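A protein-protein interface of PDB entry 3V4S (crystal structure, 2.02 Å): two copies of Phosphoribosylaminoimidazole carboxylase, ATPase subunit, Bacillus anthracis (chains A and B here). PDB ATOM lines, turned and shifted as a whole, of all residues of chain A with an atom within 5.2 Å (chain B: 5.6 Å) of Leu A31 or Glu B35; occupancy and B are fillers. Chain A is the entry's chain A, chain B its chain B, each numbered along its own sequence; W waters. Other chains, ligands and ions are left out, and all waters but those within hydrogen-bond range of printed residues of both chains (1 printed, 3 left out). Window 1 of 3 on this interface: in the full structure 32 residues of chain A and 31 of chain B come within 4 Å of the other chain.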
ATOM      1  N   GLY A  26     -21.198   5.374  19.828  1.00  0.00           N
ATOM      2  CA  GLY A  26     -20.678   5.146  21.180  1.00  0.00           C
ATOM      3  C   GLY A  26     -19.240   4.618  21.150  1.00  0.00           C
ATOM      4  O   GLY A  26     -18.391   5.062  21.926  1.00  0.00           O
ATOM      5  N   ARG A  27     -18.966   3.655  20.277  1.00  0.00           N
ATOM      6  CA  ARG A  27     -17.600   3.096  20.182  1.00  0.00           C
ATOM      7  C   ARG A  27     -16.570   4.157  19.821  1.00  0.00           C
ATOM      8  O   ARG A  27     -15.482   4.234  20.424  1.00  0.00           O
ATOM      9  CB  ARG A  27     -17.529   1.965  19.153  1.00  0.00           C
ATOM     10  CG  ARG A  27     -16.124   1.375  18.949  1.00  0.00           C
ATOM     11  CD  ARG A  27     -16.199   0.408  17.779  1.00  0.00           C
ATOM     12  NE  ARG A  27     -14.944  -0.250  17.417  1.00  0.00           N
ATOM     13  CZ  ARG A  27     -14.549  -1.438  17.889  1.00  0.00           C
ATOM     14  NH1 ARG A  27     -15.264  -2.075  18.815  1.00  0.00           N
ATOM     15  NH2 ARG A  27     -13.423  -1.987  17.435  1.00  0.00           N
ATOM     16  N   MET A  28     -16.890   4.958  18.818  1.00  0.00           N
ATOM     17  CA  MET A  28     -15.971   6.020  18.398  1.00  0.00           C
ATOM     18  C   MET A  28     -15.854   7.156  19.429  1.00  0.00           C
ATOM     19  O   MET A  28     -14.777   7.737  19.587  1.00  0.00           O
ATOM     20  CB  MET A  28     -16.340   6.512  16.994  1.00  0.00           C
ATOM     21  CG  MET A  28     -15.927   5.488  15.930  1.00  0.00           C
ATOM     22  SD  MET A  28     -16.355   5.964  14.248  1.00  0.00           S
ATOM     23  CE  MET A  28     -18.116   5.657  14.167  1.00  0.00           C
ATOM     24  N   MET A  29     -16.937   7.453  20.156  1.00  0.00           N
ATOM     25  CA  MET A  29     -16.806   8.347  21.321  1.00  0.00           C
ATOM     26  C   MET A  29     -15.824   7.767  22.349  1.00  0.00           C
ATOM     27  O   MET A  29     -15.011   8.486  22.890  1.00  0.00           O
ATOM     28  CB  MET A  29     -18.150   8.565  22.044  1.00  0.00           C
ATOM     29  CG  MET A  29     -19.230   9.312  21.274  1.00  0.00           C
ATOM     30  SD  MET A  29     -20.707   9.285  22.349  1.00  0.00           S
ATOM     31  CE  MET A  29     -21.874  10.090  21.251  1.00  0.00           C
ATOM     32  N   ALA A  30     -15.942   6.472  22.635  1.00  0.00           N
ATOM     33  CA  ALA A  30     -15.135   5.806  23.669  1.00  0.00           C
ATOM     34  C   ALA A  30     -13.645   5.779  23.294  1.00  0.00           C
ATOM     35  O   ALA A  30     -12.776   5.986  24.132  1.00  0.00           O
ATOM     36  CB  ALA A  30     -15.652   4.378  23.891  1.00  0.00           C
ATOM     37  N   LEU A  31     -13.365   5.529  22.022  1.00  0.00           N
ATOM     38  CA  LEU A  31     -11.989   5.518  21.521  1.00  0.00           C
ATOM     39  C   LEU A  31     -11.311   6.891  21.642  1.00  0.00           C
ATOM     40  O   LEU A  31     -10.164   6.981  22.079  1.00  0.00           O
ATOM     41  CB  LEU A  31     -11.950   4.992  20.075  1.00  0.00           C
ATOM     42  CG  LEU A  31     -12.280   3.494  19.937  1.00  0.00           C
ATOM     43  CD1 LEU A  31     -12.564   3.151  18.471  1.00  0.00           C
ATOM     44  CD2 LEU A  31     -11.149   2.632  20.494  1.00  0.00           C
ATOM     45  N   ALA A  32     -12.033   7.954  21.297  1.00  0.00           N
ATOM     46  CA  ALA A  32     -11.511   9.312  21.440  1.00  0.00           C
ATOM     47  C   ALA A  32     -11.320   9.637  22.917  1.00  0.00           C
ATOM     48  O   ALA A  32     -10.328  10.269  23.304  1.00  0.00           O
ATOM     49  CB  ALA A  32     -12.467  10.308  20.809  1.00  0.00           C
ATOM     50  N   ALA A  33     -12.269   9.201  23.751  1.00  0.00           N
ATOM     51  CA  ALA A  33     -12.170   9.475  25.188  1.00  0.00           C
ATOM     52  C   ALA A  33     -10.985   8.765  25.841  1.00  0.00           C
ATOM     53  O   ALA A  33     -10.352   9.317  26.741  1.00  0.00           O
ATOM     54  CB  ALA A  33     -13.468   9.105  25.892  1.00  0.00           C
ATOM     55  N   LYS A  34     -10.695   7.550  25.372  1.00  0.00           N
ATOM     56  CA  LYS A  34      -9.597   6.738  25.908  1.00  0.00           C
ATOM     57  C   LYS A  34      -8.241   7.373  25.651  1.00  0.00           C
ATOM     58  O   LYS A  34      -7.353   7.299  26.506  1.00  0.00           O
ATOM     59  CB  LYS A  34      -9.633   5.309  25.349  1.00  0.00           C
ATOM     60  CG  LYS A  34     -10.688   4.397  25.975  1.00  0.00           C
ATOM     61  CD  LYS A  34     -10.285   3.986  27.378  1.00  0.00           C
ATOM     62  CE  LYS A  34     -11.148   2.839  27.889  1.00  0.00           C
ATOM     63  NZ  LYS A  34     -10.619   2.328  29.187  1.00  0.00           N
ATOM     64  N   GLU A  35      -8.091   8.019  24.491  1.00  0.00           N
ATOM     65  CA  GLU A  35      -6.836   8.730  24.178  1.00  0.00           C
ATOM     66  C   GLU A  35      -6.563   9.782  25.233  1.00  0.00           C
ATOM     67  O   GLU A  35      -5.407  10.010  25.580  1.00  0.00           O
ATOM     68  CB  GLU A  35      -6.837   9.374  22.782  1.00  0.00           C
ATOM     69  CG  GLU A  35      -6.629   8.398  21.623  1.00  0.00           C
ATOM     70  CD  GLU A  35      -5.200   7.824  21.468  1.00  0.00           C
ATOM     71  OE1 GLU A  35      -5.049   6.953  20.556  1.00  0.00           O
ATOM     72  OE2 GLU A  35      -4.230   8.197  22.223  1.00  0.00           O
ATOM     73  N   VAL A  54     -14.816  -1.643  23.810  1.00  0.00           N
ATOM     74  CA  VAL A  54     -13.841  -0.609  24.115  1.00  0.00           C
ATOM     75  C   VAL A  54     -14.073  -0.063  25.533  1.00  0.00           C
ATOM     76  O   VAL A  54     -13.272   0.708  26.040  1.00  0.00           O
ATOM     77  CB  VAL A  54     -13.956   0.573  23.110  1.00  0.00           C
ATOM     78  CG1 VAL A  54     -13.153   1.772  23.599  1.00  0.00           C
ATOM     79  CG2 VAL A  54     -13.478   0.162  21.717  1.00  0.00           C
ATOM     80  N   GLN A 287     -12.545  12.069  11.314  1.00  0.00           N
ATOM     81  CA  GLN A 287     -11.605  11.223  12.031  1.00  0.00           C
ATOM     82  C   GLN A 287     -10.221  11.263  11.402  1.00  0.00           C
ATOM     83  O   GLN A 287      -9.214  11.175  12.104  1.00  0.00           O
ATOM     84  CB  GLN A 287     -12.055   9.780  12.026  1.00  0.00           C
ATOM     85  CG  GLN A 287     -13.239   9.447  12.917  1.00  0.00           C
ATOM     86  CD  GLN A 287     -13.394   7.952  12.956  1.00  0.00           C
ATOM     87  OE1 GLN A 287     -13.721   7.324  11.936  1.00  0.00           O
ATOM     88  NE2 GLN A 287     -13.093   7.363  14.104  1.00  0.00           N
ATOM     89  N   LEU A 341      -9.331   2.841   6.760  1.00  0.00           N
ATOM     90  CA  LEU A 341     -10.438   1.943   7.093  1.00  0.00           C
ATOM     91  C   LEU A 341     -10.869   2.017   8.563  1.00  0.00           C
ATOM     92  O   LEU A 341     -10.030   2.039   9.459  1.00  0.00           O
ATOM     93  CB  LEU A 341     -10.048   0.504   6.717  1.00  0.00           C
ATOM     94  CG  LEU A 341     -10.998  -0.656   6.974  1.00  0.00           C
ATOM     95  CD1 LEU A 341     -12.281  -0.501   6.163  1.00  0.00           C
ATOM     96  CD2 LEU A 341     -10.324  -1.981   6.642  1.00  0.00           C
ATOM     97  N   HIS A 342     -12.180   2.030   8.800  1.00  0.00           N
ATOM     98  CA  HIS A 342     -12.743   1.941  10.145  1.00  0.00           C
ATOM     99  C   HIS A 342     -13.785   0.873  10.141  1.00  0.00           C
ATOM    100  O   HIS A 342     -14.722   0.910   9.336  1.00  0.00           O
ATOM    101  CB  HIS A 342     -13.358   3.285  10.586  1.00  0.00           C
ATOM    102  CG  HIS A 342     -12.363   4.428  10.626  1.00  0.00           C
ATOM    103  ND1 HIS A 342     -11.790   4.856  11.774  1.00  0.00           N
ATOM    104  CD2 HIS A 342     -11.835   5.217   9.611  1.00  0.00           C
ATOM    105  CE1 HIS A 342     -10.941   5.879  11.510  1.00  0.00           C
ATOM    106  NE2 HIS A 342     -10.964   6.097  10.187  1.00  0.00           N
ATOM    107  N   LEU A 343     -13.627  -0.106  11.020  1.00  0.00           N
ATOM    108  CA  LEU A 343     -14.607  -1.187  11.173  1.00  0.00           C
ATOM    109  C   LEU A 343     -15.048  -1.265  12.621  1.00  0.00           C
ATOM    110  O   LEU A 343     -14.215  -1.185  13.529  1.00  0.00           O
ATOM    111  CB  LEU A 343     -14.041  -2.534  10.692  1.00  0.00           C
ATOM    112  CG  LEU A 343     -13.768  -2.659   9.170  1.00  0.00           C
ATOM    113  CD1 LEU A 343     -13.067  -3.980   8.830  1.00  0.00           C
ATOM    114  CD2 LEU A 343     -15.024  -2.502   8.326  1.00  0.00           C
ATOM    115  N   ALA B  30      -3.040  -0.562  20.366  1.00  0.00           N
ATOM    116  CA  ALA B  30      -4.351  -1.183  20.542  1.00  0.00           C
ATOM    117  C   ALA B  30      -5.490  -0.258  20.110  1.00  0.00           C
ATOM    118  O   ALA B  30      -6.415  -0.705  19.450  1.00  0.00           O
ATOM    119  CB  ALA B  30      -4.533  -1.640  21.995  1.00  0.00           C
ATOM    120  N   LEU B  31      -5.418   1.029  20.471  1.00  0.00           N
ATOM    121  CA  LEU B  31      -6.451   2.000  20.070  1.00  0.00           C
ATOM    122  C   LEU B  31      -6.514   2.179  18.547  1.00  0.00           C
ATOM    123  O   LEU B  31      -7.594   2.255  17.966  1.00  0.00           O
ATOM    124  CB  LEU B  31      -6.227   3.361  20.747  1.00  0.00           C
ATOM    125  CG  LEU B  31      -6.509   3.328  22.249  1.00  0.00           C
ATOM    126  CD1 LEU B  31      -5.858   4.509  22.957  1.00  0.00           C
ATOM    127  CD2 LEU B  31      -8.014   3.296  22.515  1.00  0.00           C
ATOM    128  N   ALA B  32      -5.347   2.234  17.911  1.00  0.00           N
ATOM    129  CA  ALA B  32      -5.259   2.350  16.457  1.00  0.00           C
ATOM    130  C   ALA B  32      -5.780   1.076  15.792  1.00  0.00           C
ATOM    131  O   ALA B  32      -6.487   1.153  14.803  1.00  0.00           O
ATOM    132  CB  ALA B  32      -3.816   2.661  16.026  1.00  0.00           C
ATOM    133  N   ALA B  33      -5.455  -0.094  16.359  1.00  0.00           N
ATOM    134  CA  ALA B  33      -5.967  -1.377  15.845  1.00  0.00           C
ATOM    135  C   ALA B  33      -7.488  -1.479  15.960  1.00  0.00           C
ATOM    136  O   ALA B  33      -8.161  -2.010  15.074  1.00  0.00           O
ATOM    137  CB  ALA B  33      -5.314  -2.536  16.579  1.00  0.00           C
ATOM    138  N   LYS B  34      -8.027  -0.988  17.073  1.00  0.00           N
ATOM    139  CA  LYS B  34      -9.467  -1.064  17.308  1.00  0.00           C
ATOM    140  C   LYS B  34     -10.274  -0.274  16.276  1.00  0.00           C
ATOM    141  O   LYS B  34     -11.377  -0.699  15.901  1.00  0.00           O
ATOM    142  CB  LYS B  34      -9.798  -0.593  18.730  1.00  0.00           C
ATOM    143  CG  LYS B  34      -9.439  -1.610  19.802  1.00  0.00           C
ATOM    144  CD  LYS B  34     -10.683  -2.335  20.266  1.00  0.00           C
ATOM    145  CE  LYS B  34     -10.381  -3.398  21.311  1.00  0.00           C
ATOM    146  NZ  LYS B  34     -11.596  -4.259  21.430  1.00  0.00           N
ATOM    147  N   GLU B  35      -9.733   0.858  15.814  1.00  0.00           N
ATOM    148  CA  GLU B  35     -10.419   1.646  14.774  1.00  0.00           C
ATOM    149  C   GLU B  35     -10.631   0.817  13.521  1.00  0.00           C
ATOM    150  O   GLU B  35     -11.673   0.930  12.872  1.00  0.00           O
ATOM    151  CB  GLU B  35      -9.677   2.935  14.418  1.00  0.00           C
ATOM    152  CG  GLU B  35      -9.814   4.044  15.458  1.00  0.00           C
ATOM    153  CD  GLU B  35     -11.176   4.765  15.507  1.00  0.00           C
ATOM    154  OE1 GLU B  35     -12.155   4.444  14.723  1.00  0.00           O
ATOM    155  OE2 GLU B  35     -11.271   5.686  16.385  1.00  0.00           O
ATOM    156  N   MET B  36      -9.646  -0.032  13.201  1.00  0.00           N
ATOM    157  CA  MET B  36      -9.757  -0.926  12.054  1.00  0.00           C
ATOM    158  C   MET B  36     -10.536  -2.214  12.310  1.00  0.00           C
ATOM    159  O   MET B  36     -10.694  -3.010  11.395  1.00  0.00           O
ATOM    160  CB  MET B  36      -8.377  -1.238  11.467  1.00  0.00           C
ATOM    161  CG  MET B  36      -7.756  -0.042  10.776  1.00  0.00           C
ATOM    162  SD  MET B  36      -6.105  -0.318  10.097  1.00  0.00           S
ATOM    163  CE  MET B  36      -5.158  -0.426  11.607  1.00  0.00           C
ATOM    164  N   GLY B  37     -11.018  -2.415  13.534  1.00  0.00           N
ATOM    165  CA  GLY B  37     -11.829  -3.583  13.889  1.00  0.00           C
ATOM    166  C   GLY B  37     -11.069  -4.847  14.294  1.00  0.00           C
ATOM    167  O   GLY B  37     -11.639  -5.941  14.304  1.00  0.00           O
ATOM    168  N   VAL B  54      -7.682  -1.206  27.233  1.00  0.00           N
ATOM    169  CA  VAL B  54      -8.230  -1.079  25.884  1.00  0.00           C
ATOM    170  C   VAL B  54      -8.248  -2.424  25.140  1.00  0.00           C
ATOM    171  O   VAL B  54      -8.660  -2.498  23.991  1.00  0.00           O
ATOM    172  CB  VAL B  54      -7.466   0.002  25.071  1.00  0.00           C
ATOM    173  CG1 VAL B  54      -5.980  -0.287  25.044  1.00  0.00           C
ATOM    174  CG2 VAL B  54      -7.986   0.069  23.651  1.00  0.00           C
HETATM  175  O   HOH W   1     -12.287  -4.455  18.132  1.00  0.00           O
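Leu B31 touches its own counterpart, Leu A31.
Leu A31 touches Lys B34, and with the chains exchanged Lys A34 touches Leu B31.
Leu A31 touches Glu B35, and with the chains exchanged Glu A35 touches Leu B31.
Positions printed for both chains: 30, 31, 32, 33, 34, 35 and 54.
Water W1 bridges the guanidinium group of Arg A27 (2.8 Å) and the side-chain amino group of Lys B34 (3.4 Å).
NE2 of Gln A287 lies within hydrogen-bond range of SD of Met A28, 3.6 Å away.
The side-chain amide oxygen (OE1) of Gln A287 sits at hydrogen-bond distance from a ring nitrogen (ND1) of His A342 (3.1 Å).
Leu A31 touches Leu B31.
Lys B34 touches Leu A31 (CB to CD2, 3.9 Å).
Glu B35 touches Leu A31 (OE2 to CD1, 3.5 Å).
Leu B31 touches Lys A34 (CD2 to CB, 3.8 Å).
Glu A35 touches Leu B31.
Glu B35 touches Leu A341 (O to O, 3.9 Å).
CG of Met B36 touches O of Leu A341, at 3.4 Å.
O of Leu A343 touches O of Lys B34, at 3.7 Å.
Met B36 touches Leu A343 (O to CB, 3.5 Å).
Printed residues of chain B that touch a printed residue of chain A: Leu B31, Lys B34, Glu B35, Met B36 and Gly B37.
Along chain B the printed residues that touch a printed residue of chain A span positions 31 to 37.
Of the 15 printed residues of chain A, 8 touch a printed residue of chain B.
Hydrophobic or aromatic side chains of chain A within 4 Å of the printed part of chain B: Leu A31, His A342 and Leu A343.
Along chain A the printed residues that touch a printed residue of chain B span positions 27 to 343.
Among the printed residues, 14 pairs touch across the chains.
Among the printed residues, no Asp or Glu carboxylate lies within 4 Å of a Lys or Arg side-chain nitrogen of the other chain.
Of chain B, only Leu B31, Lys B34 and Glu B35 come within 4 Å of Leu A31.
Of chain A, only Leu A31 (3.5 Å), Gln A287 (3.1 Å), Leu A341 (3.9 Å), His A342 (3.0 Å) and Leu A343 (2.9 Å) come within 4 Å of Glu B35.
Of the printed residues of chain B, Arg A27 touches Lys B34 (2.9 Å).
Of the printed residues of chain A, Lys B34 touches Arg A27, Leu A31 and Leu A343.
Ala A33 touches none of the printed residues of chain B.
Ala A32 touches none of the printed residues of chain B.
The nearest printed residue of chain B that does not touch Gln A287 is Met B36 (8.2 Å).
The guanidinium group (NH2) of Arg A27 is in hydrogen-bond range of the backbone carbonyl oxygen (O) of Lys B34 (2.9 Å).
The side-chain amide nitrogen of Gln A287 lies within hydrogen-bond range of the side-chain carboxylate of Glu B35, 3.1 Å away.
OE1 of Glu B35 is in hydrogen-bond range of ND1 of His A342, 3.0 Å away.
The backbone carbonyl oxygen (O) of Glu B35 is in hydrogen-bond range of the backbone NH (N) of Leu A343 (2.9 Å).
The backbone carbonyl oxygen of Leu A343 sits close to the backbone NH of Gly B37 (3.4 Å).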
